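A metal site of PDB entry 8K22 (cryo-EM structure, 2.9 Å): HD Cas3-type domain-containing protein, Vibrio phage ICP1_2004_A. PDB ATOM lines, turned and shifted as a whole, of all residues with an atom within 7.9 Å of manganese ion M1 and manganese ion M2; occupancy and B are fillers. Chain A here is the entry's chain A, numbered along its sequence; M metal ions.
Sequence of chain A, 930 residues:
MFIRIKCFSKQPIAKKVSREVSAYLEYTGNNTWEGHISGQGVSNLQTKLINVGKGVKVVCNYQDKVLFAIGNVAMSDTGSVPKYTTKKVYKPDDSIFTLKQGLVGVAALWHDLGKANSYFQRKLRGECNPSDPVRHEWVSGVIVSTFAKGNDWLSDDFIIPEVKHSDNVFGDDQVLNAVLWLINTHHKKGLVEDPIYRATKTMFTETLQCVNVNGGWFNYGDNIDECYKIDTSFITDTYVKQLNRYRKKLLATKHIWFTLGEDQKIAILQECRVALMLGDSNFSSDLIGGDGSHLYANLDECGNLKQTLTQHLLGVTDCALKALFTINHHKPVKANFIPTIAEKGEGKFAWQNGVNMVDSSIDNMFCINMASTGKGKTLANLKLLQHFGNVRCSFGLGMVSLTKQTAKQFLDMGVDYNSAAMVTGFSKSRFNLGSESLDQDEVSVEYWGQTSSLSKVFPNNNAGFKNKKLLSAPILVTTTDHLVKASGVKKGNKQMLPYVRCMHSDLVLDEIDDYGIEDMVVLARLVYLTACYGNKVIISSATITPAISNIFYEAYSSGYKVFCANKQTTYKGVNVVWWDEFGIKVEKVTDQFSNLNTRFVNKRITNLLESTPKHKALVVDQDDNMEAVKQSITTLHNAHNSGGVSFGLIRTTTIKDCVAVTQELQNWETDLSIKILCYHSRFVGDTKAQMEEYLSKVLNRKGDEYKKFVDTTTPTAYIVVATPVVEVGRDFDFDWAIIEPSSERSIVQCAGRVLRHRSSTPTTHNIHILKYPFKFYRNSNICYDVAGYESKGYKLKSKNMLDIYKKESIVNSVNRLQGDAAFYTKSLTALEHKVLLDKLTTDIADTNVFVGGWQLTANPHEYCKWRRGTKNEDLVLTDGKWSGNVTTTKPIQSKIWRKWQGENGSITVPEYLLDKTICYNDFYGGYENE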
ATOM      1  N   ALA A 108      -6.139  -1.497  23.934  1.00  0.00           N
ATOM      2  CA  ALA A 108      -5.840  -1.163  25.323  1.00  0.00           C
ATOM      3  C   ALA A 108      -5.173  -2.333  26.050  1.00  0.00           C
ATOM      4  O   ALA A 108      -4.446  -2.114  27.027  1.00  0.00           O
ATOM      5  CB  ALA A 108      -7.113  -0.743  26.044  1.00  0.00           C
ATOM      6  N   HIS A 111      -1.608  -1.647  24.498  1.00  0.00           N
ATOM      7  CA  HIS A 111      -1.091  -0.289  24.455  1.00  0.00           C
ATOM      8  C   HIS A 111       0.206  -0.135  25.222  1.00  0.00           C
ATOM      9  O   HIS A 111       0.997   0.779  24.928  1.00  0.00           O
ATOM     10  CB  HIS A 111      -2.137   0.693  24.996  1.00  0.00           C
ATOM     11  CG  HIS A 111      -2.095   0.879  26.483  1.00  0.00           C
ATOM     12  ND1 HIS A 111      -2.292  -0.157  27.364  1.00  0.00           N
ATOM     13  CD2 HIS A 111      -1.891   1.982  27.243  1.00  0.00           C
ATOM     14  CE1 HIS A 111      -2.192   0.283  28.601  1.00  0.00           C
ATOM     15  NE2 HIS A 111      -1.961   1.585  28.558  1.00  0.00           N
ATOM     16  N   ASP A 112       0.478  -1.002  26.193  1.00  0.00           N
ATOM     17  CA  ASP A 112       1.658  -0.904  27.029  1.00  0.00           C
ATOM     18  C   ASP A 112       2.434  -2.217  27.042  1.00  0.00           C
ATOM     19  O   ASP A 112       2.982  -2.620  28.063  1.00  0.00           O
ATOM     20  CB  ASP A 112       1.293  -0.473  28.449  1.00  0.00           C
ATOM     21  CG  ASP A 112       1.187   1.028  28.586  1.00  0.00           C
ATOM     22  OD1 ASP A 112       1.532   1.751  27.635  1.00  0.00           O
ATOM     23  OD2 ASP A 112       0.756   1.499  29.665  1.00  0.00           O
ATOM     24  N   LEU A 113       2.472  -2.895  25.904  1.00  0.00           N
ATOM     25  CA  LEU A 113       3.310  -4.085  25.789  1.00  0.00           C
ATOM     26  C   LEU A 113       4.786  -3.714  25.718  1.00  0.00           C
ATOM     27  O   LEU A 113       5.653  -4.549  26.025  1.00  0.00           O
ATOM     28  CB  LEU A 113       2.922  -4.895  24.568  1.00  0.00           C
ATOM     29  CG  LEU A 113       1.616  -5.690  24.592  1.00  0.00           C
ATOM     30  CD1 LEU A 113       1.369  -6.273  23.219  1.00  0.00           C
ATOM     31  CD2 LEU A 113       1.696  -6.784  25.630  1.00  0.00           C
ATOM     32  N   LYS A 115       6.479  -1.539  27.487  1.00  0.00           N
ATOM     33  CA  LYS A 115       7.166  -1.237  28.734  1.00  0.00           C
ATOM     34  C   LYS A 115       7.892  -2.442  29.310  1.00  0.00           C
ATOM     35  O   LYS A 115       8.571  -2.300  30.334  1.00  0.00           O
ATOM     36  CB  LYS A 115       6.189  -0.704  29.791  1.00  0.00           C
ATOM     37  CG  LYS A 115       5.611   0.655  29.506  1.00  0.00           C
ATOM     38  CD  LYS A 115       4.588   1.028  30.545  1.00  0.00           C
ATOM     39  CE  LYS A 115       3.957   2.373  30.248  1.00  0.00           C
ATOM     40  NZ  LYS A 115       2.729   2.609  31.037  1.00  0.00           N
ATOM     41  N   PHE A 120      12.884   0.146  30.028  1.00  0.00           N
ATOM     42  CA  PHE A 120      11.817   0.729  30.831  1.00  0.00           C
ATOM     43  C   PHE A 120      11.866   0.243  32.271  1.00  0.00           C
ATOM     44  O   PHE A 120      11.490   0.987  33.186  1.00  0.00           O
ATOM     45  CB  PHE A 120      10.454   0.411  30.222  1.00  0.00           C
ATOM     46  CG  PHE A 120       9.413   1.444  30.488  1.00  0.00           C
ATOM     47  CD1 PHE A 120       8.648   1.399  31.643  1.00  0.00           C
ATOM     48  CD2 PHE A 120       9.189   2.484  29.588  1.00  0.00           C
ATOM     49  CE1 PHE A 120       7.690   2.363  31.901  1.00  0.00           C
ATOM     50  CE2 PHE A 120       8.233   3.443  29.837  1.00  0.00           C
ATOM     51  CZ  PHE A 120       7.477   3.376  30.998  1.00  0.00           C
ATOM     52  N   ARG A 135       9.962   5.248  22.247  1.00  0.00           N
ATOM     53  CA  ARG A 135       8.863   5.274  23.200  1.00  0.00           C
ATOM     54  C   ARG A 135       8.167   3.918  23.233  1.00  0.00           C
ATOM     55  O   ARG A 135       8.107   3.199  22.232  1.00  0.00           O
ATOM     56  CB  ARG A 135       7.872   6.375  22.838  1.00  0.00           C
ATOM     57  CG  ARG A 135       8.495   7.760  22.758  1.00  0.00           C
ATOM     58  CD  ARG A 135       7.436   8.843  22.785  1.00  0.00           C
ATOM     59  NE  ARG A 135       6.448   8.608  23.836  1.00  0.00           N
ATOM     60  CZ  ARG A 135       6.572   9.028  25.080  1.00  0.00           C
ATOM     61  NH1 ARG A 135       7.625   9.732  25.476  1.00  0.00           N
ATOM     62  NH2 ARG A 135       5.612   8.747  25.958  1.00  0.00           N
ATOM     63  N   HIS A 136       7.630   3.581  24.418  1.00  0.00           N
ATOM     64  CA  HIS A 136       7.088   2.248  24.651  1.00  0.00           C
ATOM     65  C   HIS A 136       5.827   1.975  23.840  1.00  0.00           C
ATOM     66  O   HIS A 136       5.510   0.804  23.596  1.00  0.00           O
ATOM     67  CB  HIS A 136       6.778   2.071  26.137  1.00  0.00           C
ATOM     68  CG  HIS A 136       5.740   3.018  26.655  1.00  0.00           C
ATOM     69  ND1 HIS A 136       6.048   4.242  27.196  1.00  0.00           N
ATOM     70  CD2 HIS A 136       4.390   2.906  26.711  1.00  0.00           C
ATOM     71  CE1 HIS A 136       4.944   4.854  27.559  1.00  0.00           C
ATOM     72  NE2 HIS A 136       3.917   4.070  27.276  1.00  0.00           N
ATOM     73  N   GLU A 137       5.107   3.022  23.418  1.00  0.00           N
ATOM     74  CA  GLU A 137       3.983   2.832  22.509  1.00  0.00           C
ATOM     75  C   GLU A 137       4.453   2.284  21.169  1.00  0.00           C
ATOM     76  O   GLU A 137       3.821   1.395  20.598  1.00  0.00           O
ATOM     77  CB  GLU A 137       3.213   4.135  22.329  1.00  0.00           C
ATOM     78  CG  GLU A 137       4.072   5.367  22.191  1.00  0.00           C
ATOM     79  CD  GLU A 137       4.234   6.121  23.486  1.00  0.00           C
ATOM     80  OE1 GLU A 137       4.160   5.490  24.558  1.00  0.00           O
ATOM     81  OE2 GLU A 137       4.433   7.360  23.433  1.00  0.00           O
ATOM     82  N   SER A 140       5.455  -1.422  21.705  1.00  0.00           N
ATOM     83  CA  SER A 140       4.257  -2.260  21.705  1.00  0.00           C
ATOM     84  C   SER A 140       3.661  -2.388  20.311  1.00  0.00           C
ATOM     85  O   SER A 140       3.142  -3.447  19.948  1.00  0.00           O
ATOM     86  CB  SER A 140       3.231  -1.696  22.680  1.00  0.00           C
ATOM     87  OG  SER A 140       3.013  -0.322  22.451  1.00  0.00           O
ATOM     88  N   ILE A 183      -2.490   1.970  19.243  1.00  0.00           N
ATOM     89  CA  ILE A 183      -1.415   1.598  20.152  1.00  0.00           C
ATOM     90  C   ILE A 183      -0.326   2.665  20.165  1.00  0.00           C
ATOM     91  O   ILE A 183       0.116   3.111  21.223  1.00  0.00           O
ATOM     92  CB  ILE A 183      -0.850   0.219  19.761  1.00  0.00           C
ATOM     93  CG1 ILE A 183      -1.793  -0.895  20.210  1.00  0.00           C
ATOM     94  CG2 ILE A 183       0.521  -0.017  20.351  1.00  0.00           C
ATOM     95  CD1 ILE A 183      -1.614  -2.133  19.407  1.00  0.00           C
ATOM     96  N   HIS A 186      -1.384   6.422  21.671  1.00  0.00           N
ATOM     97  CA  HIS A 186      -2.071   6.503  22.949  1.00  0.00           C
ATOM     98  C   HIS A 186      -1.419   7.504  23.892  1.00  0.00           C
ATOM     99  O   HIS A 186      -1.953   7.749  24.978  1.00  0.00           O
ATOM    100  CB  HIS A 186      -2.145   5.112  23.586  1.00  0.00           C
ATOM    101  CG  HIS A 186      -1.008   4.791  24.508  1.00  0.00           C
ATOM    102  ND1 HIS A 186       0.203   4.321  24.049  1.00  0.00           N
ATOM    103  CD2 HIS A 186      -0.908   4.859  25.853  1.00  0.00           C
ATOM    104  CE1 HIS A 186       1.007   4.121  25.071  1.00  0.00           C
ATOM    105  NE2 HIS A 186       0.362   4.425  26.180  1.00  0.00           N
ATOM    106  N   HIS A 187      -0.275   8.078  23.511  1.00  0.00           N
ATOM    107  CA  HIS A 187       0.325   9.194  24.223  1.00  0.00           C
ATOM    108  C   HIS A 187       0.469  10.432  23.347  1.00  0.00           C
ATOM    109  O   HIS A 187       0.095  11.531  23.777  1.00  0.00           O
ATOM    110  CB  HIS A 187       1.701   8.795  24.795  1.00  0.00           C
ATOM    111  CG  HIS A 187       1.612   8.133  26.137  1.00  0.00           C
ATOM    112  ND1 HIS A 187       2.328   6.983  26.446  1.00  0.00           N
ATOM    113  CD2 HIS A 187       0.909   8.446  27.242  1.00  0.00           C
ATOM    114  CE1 HIS A 187       2.068   6.637  27.688  1.00  0.00           C
ATOM    115  NE2 HIS A 187       1.201   7.505  28.195  1.00  0.00           N
ATOM    116  N   LEU A 276      -9.315   5.797  24.720  1.00  0.00           N
ATOM    117  CA  LEU A 276      -8.132   5.084  25.172  1.00  0.00           C
ATOM    118  C   LEU A 276      -7.278   5.941  26.095  1.00  0.00           C
ATOM    119  O   LEU A 276      -6.765   5.444  27.103  1.00  0.00           O
ATOM    120  CB  LEU A 276      -7.329   4.591  23.966  1.00  0.00           C
ATOM    121  CG  LEU A 276      -5.981   3.922  24.217  1.00  0.00           C
ATOM    122  CD1 LEU A 276      -6.131   2.768  25.181  1.00  0.00           C
ATOM    123  CD2 LEU A 276      -5.434   3.416  22.898  1.00  0.00           C
ATOM    124  N   GLY A 279      -9.223   6.066  29.485  1.00  0.00           N
ATOM    125  CA  GLY A 279      -8.988   4.903  30.314  1.00  0.00           C
ATOM    126  C   GLY A 279      -7.571   4.812  30.844  1.00  0.00           C
ATOM    127  O   GLY A 279      -7.348   4.451  32.000  1.00  0.00           O
ATOM    128  N   ASP A 280      -6.581   5.164  30.008  1.00  0.00           N
ATOM    129  CA  ASP A 280      -5.188   5.102  30.413  1.00  0.00           C
ATOM    130  C   ASP A 280      -4.870   6.102  31.506  1.00  0.00           C
ATOM    131  O   ASP A 280      -4.238   5.758  32.513  1.00  0.00           O
ATOM    132  CB  ASP A 280      -4.272   5.315  29.201  1.00  0.00           C
ATOM    133  CG  ASP A 280      -2.803   5.210  29.550  1.00  0.00           C
ATOM    134  OD1 ASP A 280      -2.451   4.321  30.352  1.00  0.00           O
ATOM    135  OD2 ASP A 280      -2.013   6.007  29.016  1.00  0.00           O
ATOM    136  N   SER A 281      -5.338   7.341  31.354  1.00  0.00           N
ATOM    137  CA  SER A 281      -5.097   8.352  32.389  1.00  0.00           C
ATOM    138  C   SER A 281      -5.942   8.086  33.628  1.00  0.00           C
ATOM    139  O   SER A 281      -5.509   8.422  34.740  1.00  0.00           O
ATOM    140  CB  SER A 281      -5.386   9.742  31.823  1.00  0.00           C
ATOM    141  OG  SER A 281      -6.589   9.748  31.081  1.00  0.00           O
ATOM    142  N   PHE A 283      -6.701   5.063  34.816  1.00  0.00           N
ATOM    143  CA  PHE A 283      -6.025   4.036  35.602  1.00  0.00           C
ATOM    144  C   PHE A 283      -4.645   4.488  36.080  1.00  0.00           C
ATOM    145  O   PHE A 283      -4.169   3.992  37.106  1.00  0.00           O
ATOM    146  CB  PHE A 283      -5.902   2.737  34.808  1.00  0.00           C
ATOM    147  CG  PHE A 283      -5.774   1.541  35.691  1.00  0.00           C
ATOM    148  CD1 PHE A 283      -6.796   1.197  36.566  1.00  0.00           C
ATOM    149  CD2 PHE A 283      -4.626   0.764  35.671  1.00  0.00           C
ATOM    150  CE1 PHE A 283      -6.678   0.098  37.389  1.00  0.00           C
ATOM    151  CE2 PHE A 283      -4.510  -0.330  36.502  1.00  0.00           C
ATOM    152  CZ  PHE A 283      -5.531  -0.668  37.360  1.00  0.00           C
ATOM    153  N   SER A 284      -3.995   5.404  35.358  1.00  0.00           N
ATOM    154  CA  SER A 284      -2.709   5.916  35.811  1.00  0.00           C
ATOM    155  C   SER A 284      -2.841   6.931  36.937  1.00  0.00           C
ATOM    156  O   SER A 284      -1.867   7.152  37.670  1.00  0.00           O
ATOM    157  CB  SER A 284      -1.944   6.534  34.639  1.00  0.00           C
ATOM    158  OG  SER A 284      -1.439   5.531  33.775  1.00  0.00           O
ATOM    159  N   ALA A 297       4.728  -0.817  35.309  1.00  0.00           N
ATOM    160  CA  ALA A 297       4.313   0.157  34.309  1.00  0.00           C
ATOM    161  C   ALA A 297       4.539   1.594  34.742  1.00  0.00           C
ATOM    162  O   ALA A 297       5.204   2.354  34.036  1.00  0.00           O
ATOM    163  CB  ALA A 297       2.825  -0.039  33.975  1.00  0.00           C
ATOM    164  N   ASN A 298       3.994   1.984  35.883  1.00  0.00           N
ATOM    165  CA  ASN A 298       3.998   3.375  36.309  1.00  0.00           C
ATOM    166  C   ASN A 298       4.669   3.502  37.667  1.00  0.00           C
ATOM    167  O   ASN A 298       4.989   2.511  38.337  1.00  0.00           O
ATOM    168  CB  ASN A 298       2.574   3.930  36.365  1.00  0.00           C
ATOM    169  CG  ASN A 298       1.686   3.367  35.271  1.00  0.00           C
ATOM    170  OD1 ASN A 298       0.822   2.529  35.522  1.00  0.00           O
ATOM    171  ND2 ASN A 298       1.906   3.819  34.044  1.00  0.00           N
ATOM    172  N   GLN A 307       1.678  -0.745  40.196  1.00  0.00           N
ATOM    173  CA  GLN A 307       0.883  -0.969  38.985  1.00  0.00           C
ATOM    174  C   GLN A 307       1.626  -1.869  37.990  1.00  0.00           C
ATOM    175  O   GLN A 307       2.118  -1.412  36.947  1.00  0.00           O
ATOM    176  CB  GLN A 307       0.454   0.344  38.335  1.00  0.00           C
ATOM    177  CG  GLN A 307      -0.999   0.683  38.545  1.00  0.00           C
ATOM    178  CD  GLN A 307      -1.334   2.105  38.146  1.00  0.00           C
ATOM    179  OE1 GLN A 307      -0.463   2.974  38.125  1.00  0.00           O
ATOM    180  NE2 GLN A 307      -2.597   2.347  37.834  1.00  0.00           N
ATOM    181  N   LEU A 309       2.321  -4.643  35.136  1.00  0.00           N
ATOM    182  CA  LEU A 309       1.892  -4.336  33.768  1.00  0.00           C
ATOM    183  C   LEU A 309       0.699  -5.179  33.335  1.00  0.00           C
ATOM    184  O   LEU A 309      -0.086  -4.719  32.491  1.00  0.00           O
ATOM    185  CB  LEU A 309       3.068  -4.526  32.811  1.00  0.00           C
ATOM    186  CG  LEU A 309       2.984  -3.927  31.408  1.00  0.00           C
ATOM    187  CD1 LEU A 309       2.243  -2.604  31.369  1.00  0.00           C
ATOM    188  CD2 LEU A 309       4.392  -3.773  30.856  1.00  0.00           C
ATOM    189  N   HIS A 312      -2.086  -3.474  35.041  1.00  0.00           N
ATOM    190  CA  HIS A 312      -2.162  -2.146  34.434  1.00  0.00           C
ATOM    191  C   HIS A 312      -2.867  -2.191  33.083  1.00  0.00           C
ATOM    192  O   HIS A 312      -3.710  -1.340  32.794  1.00  0.00           O
ATOM    193  CB  HIS A 312      -0.763  -1.551  34.260  1.00  0.00           C
ATOM    194  CG  HIS A 312      -0.755  -0.297  33.447  1.00  0.00           C
ATOM    195  ND1 HIS A 312      -1.261   0.899  33.907  1.00  0.00           N
ATOM    196  CD2 HIS A 312      -0.312  -0.064  32.183  1.00  0.00           C
ATOM    197  CE1 HIS A 312      -1.128   1.818  32.974  1.00  0.00           C
ATOM    198  NE2 HIS A 312      -0.549   1.265  31.920  1.00  0.00           N
ATOM    199  N   LEU A 313      -2.516  -3.182  32.244  1.00  0.00           N
ATOM    200  CA  LEU A 313      -3.187  -3.342  30.960  1.00  0.00           C
ATOM    201  C   LEU A 313      -4.655  -3.673  31.141  1.00  0.00           C
ATOM    202  O   LEU A 313      -5.518  -3.140  30.429  1.00  0.00           O
ATOM    203  CB  LEU A 313      -2.499  -4.432  30.143  1.00  0.00           C
ATOM    204  CG  LEU A 313      -1.185  -4.063  29.442  1.00  0.00           C
ATOM    205  CD1 LEU A 313      -0.357  -5.310  29.204  1.00  0.00           C
ATOM    206  CD2 LEU A 313      -1.460  -3.345  28.142  1.00  0.00           C
ATOM    207  N   VAL A 316      -6.449  -0.415  32.386  1.00  0.00           N
ATOM    208  CA  VAL A 316      -6.611   0.537  31.299  1.00  0.00           C
ATOM    209  C   VAL A 316      -7.677   0.055  30.313  1.00  0.00           C
ATOM    210  O   VAL A 316      -8.504   0.839  29.850  1.00  0.00           O
ATOM    211  CB  VAL A 316      -5.251   0.791  30.603  1.00  0.00           C
ATOM    212  CG1 VAL A 316      -5.416   1.507  29.274  1.00  0.00           C
ATOM    213  CG2 VAL A 316      -4.360   1.606  31.514  1.00  0.00           C
HETATM  214 MN    MN M   1      -0.869   2.825  30.235  1.00  0.00          MN
HETATM  215 MN    MN M   2       1.729   4.198  27.990  1.00  0.00          MN
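The side-chain amino group of Lys 115 lies close to the side-chain carboxylate of Asp 112 (2.6 Å). O of Asp 280 sits at hydrogen-bond distance from OG of Ser 284 (3.1 Å). ND1 of His 186 is in hydrogen-bond range of O of Ile 183, at 3.1 Å. A ring nitrogen (NE2) of His 136 sits close to a ring nitrogen (ND1) of His 187. The backbone carbonyl oxygen (O) of His 136 sits at hydrogen-bond distance from the side-chain hydroxyl (OG) of Ser 140 (3.0 Å). A ring nitrogen (ND1) of His 312 sits at hydrogen-bond distance from the side-chain amide oxygen (OD1) of Asn 298 (3.1 Å). ND1 of His 111 is in hydrogen-bond range of O of Ala 108, 2.9 Å away. ND1 of His 187 sits at hydrogen-bond distance from OE1 of Glu 137 (3.0 Å).
Residues that only touch manganese ion M1: Lys 115 (3.7 Å) and Val 316 (3.9 Å). Six residues have an atom within 4 Å of manganese ion M1: His 111, Asp 112, Lys 115, Asp 280, His 312 and Val 316.
Merely in contact with manganese ion M2: Lys 115 (3.6 Å) and His 187 (2.5 Å). Within 4 Å of manganese ion M2: Asp 112, Lys 115, His 136, His 186 and His 187.
Manganese ion M1 is bound by OD2 of Asp 112, OD1 of Asp 280, NE2 of His 312 and NE2 of His 111. Manganese ion M1 has four donor atoms within binding distance.
Manganese ion M2 is bound by NE2 of His 186 (2.3 Å), NE2 of His 136 (2.3 Å) and OD1 of Asp 112 (2.5 Å). Manganese ion M2 has three donor atoms within binding distance.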
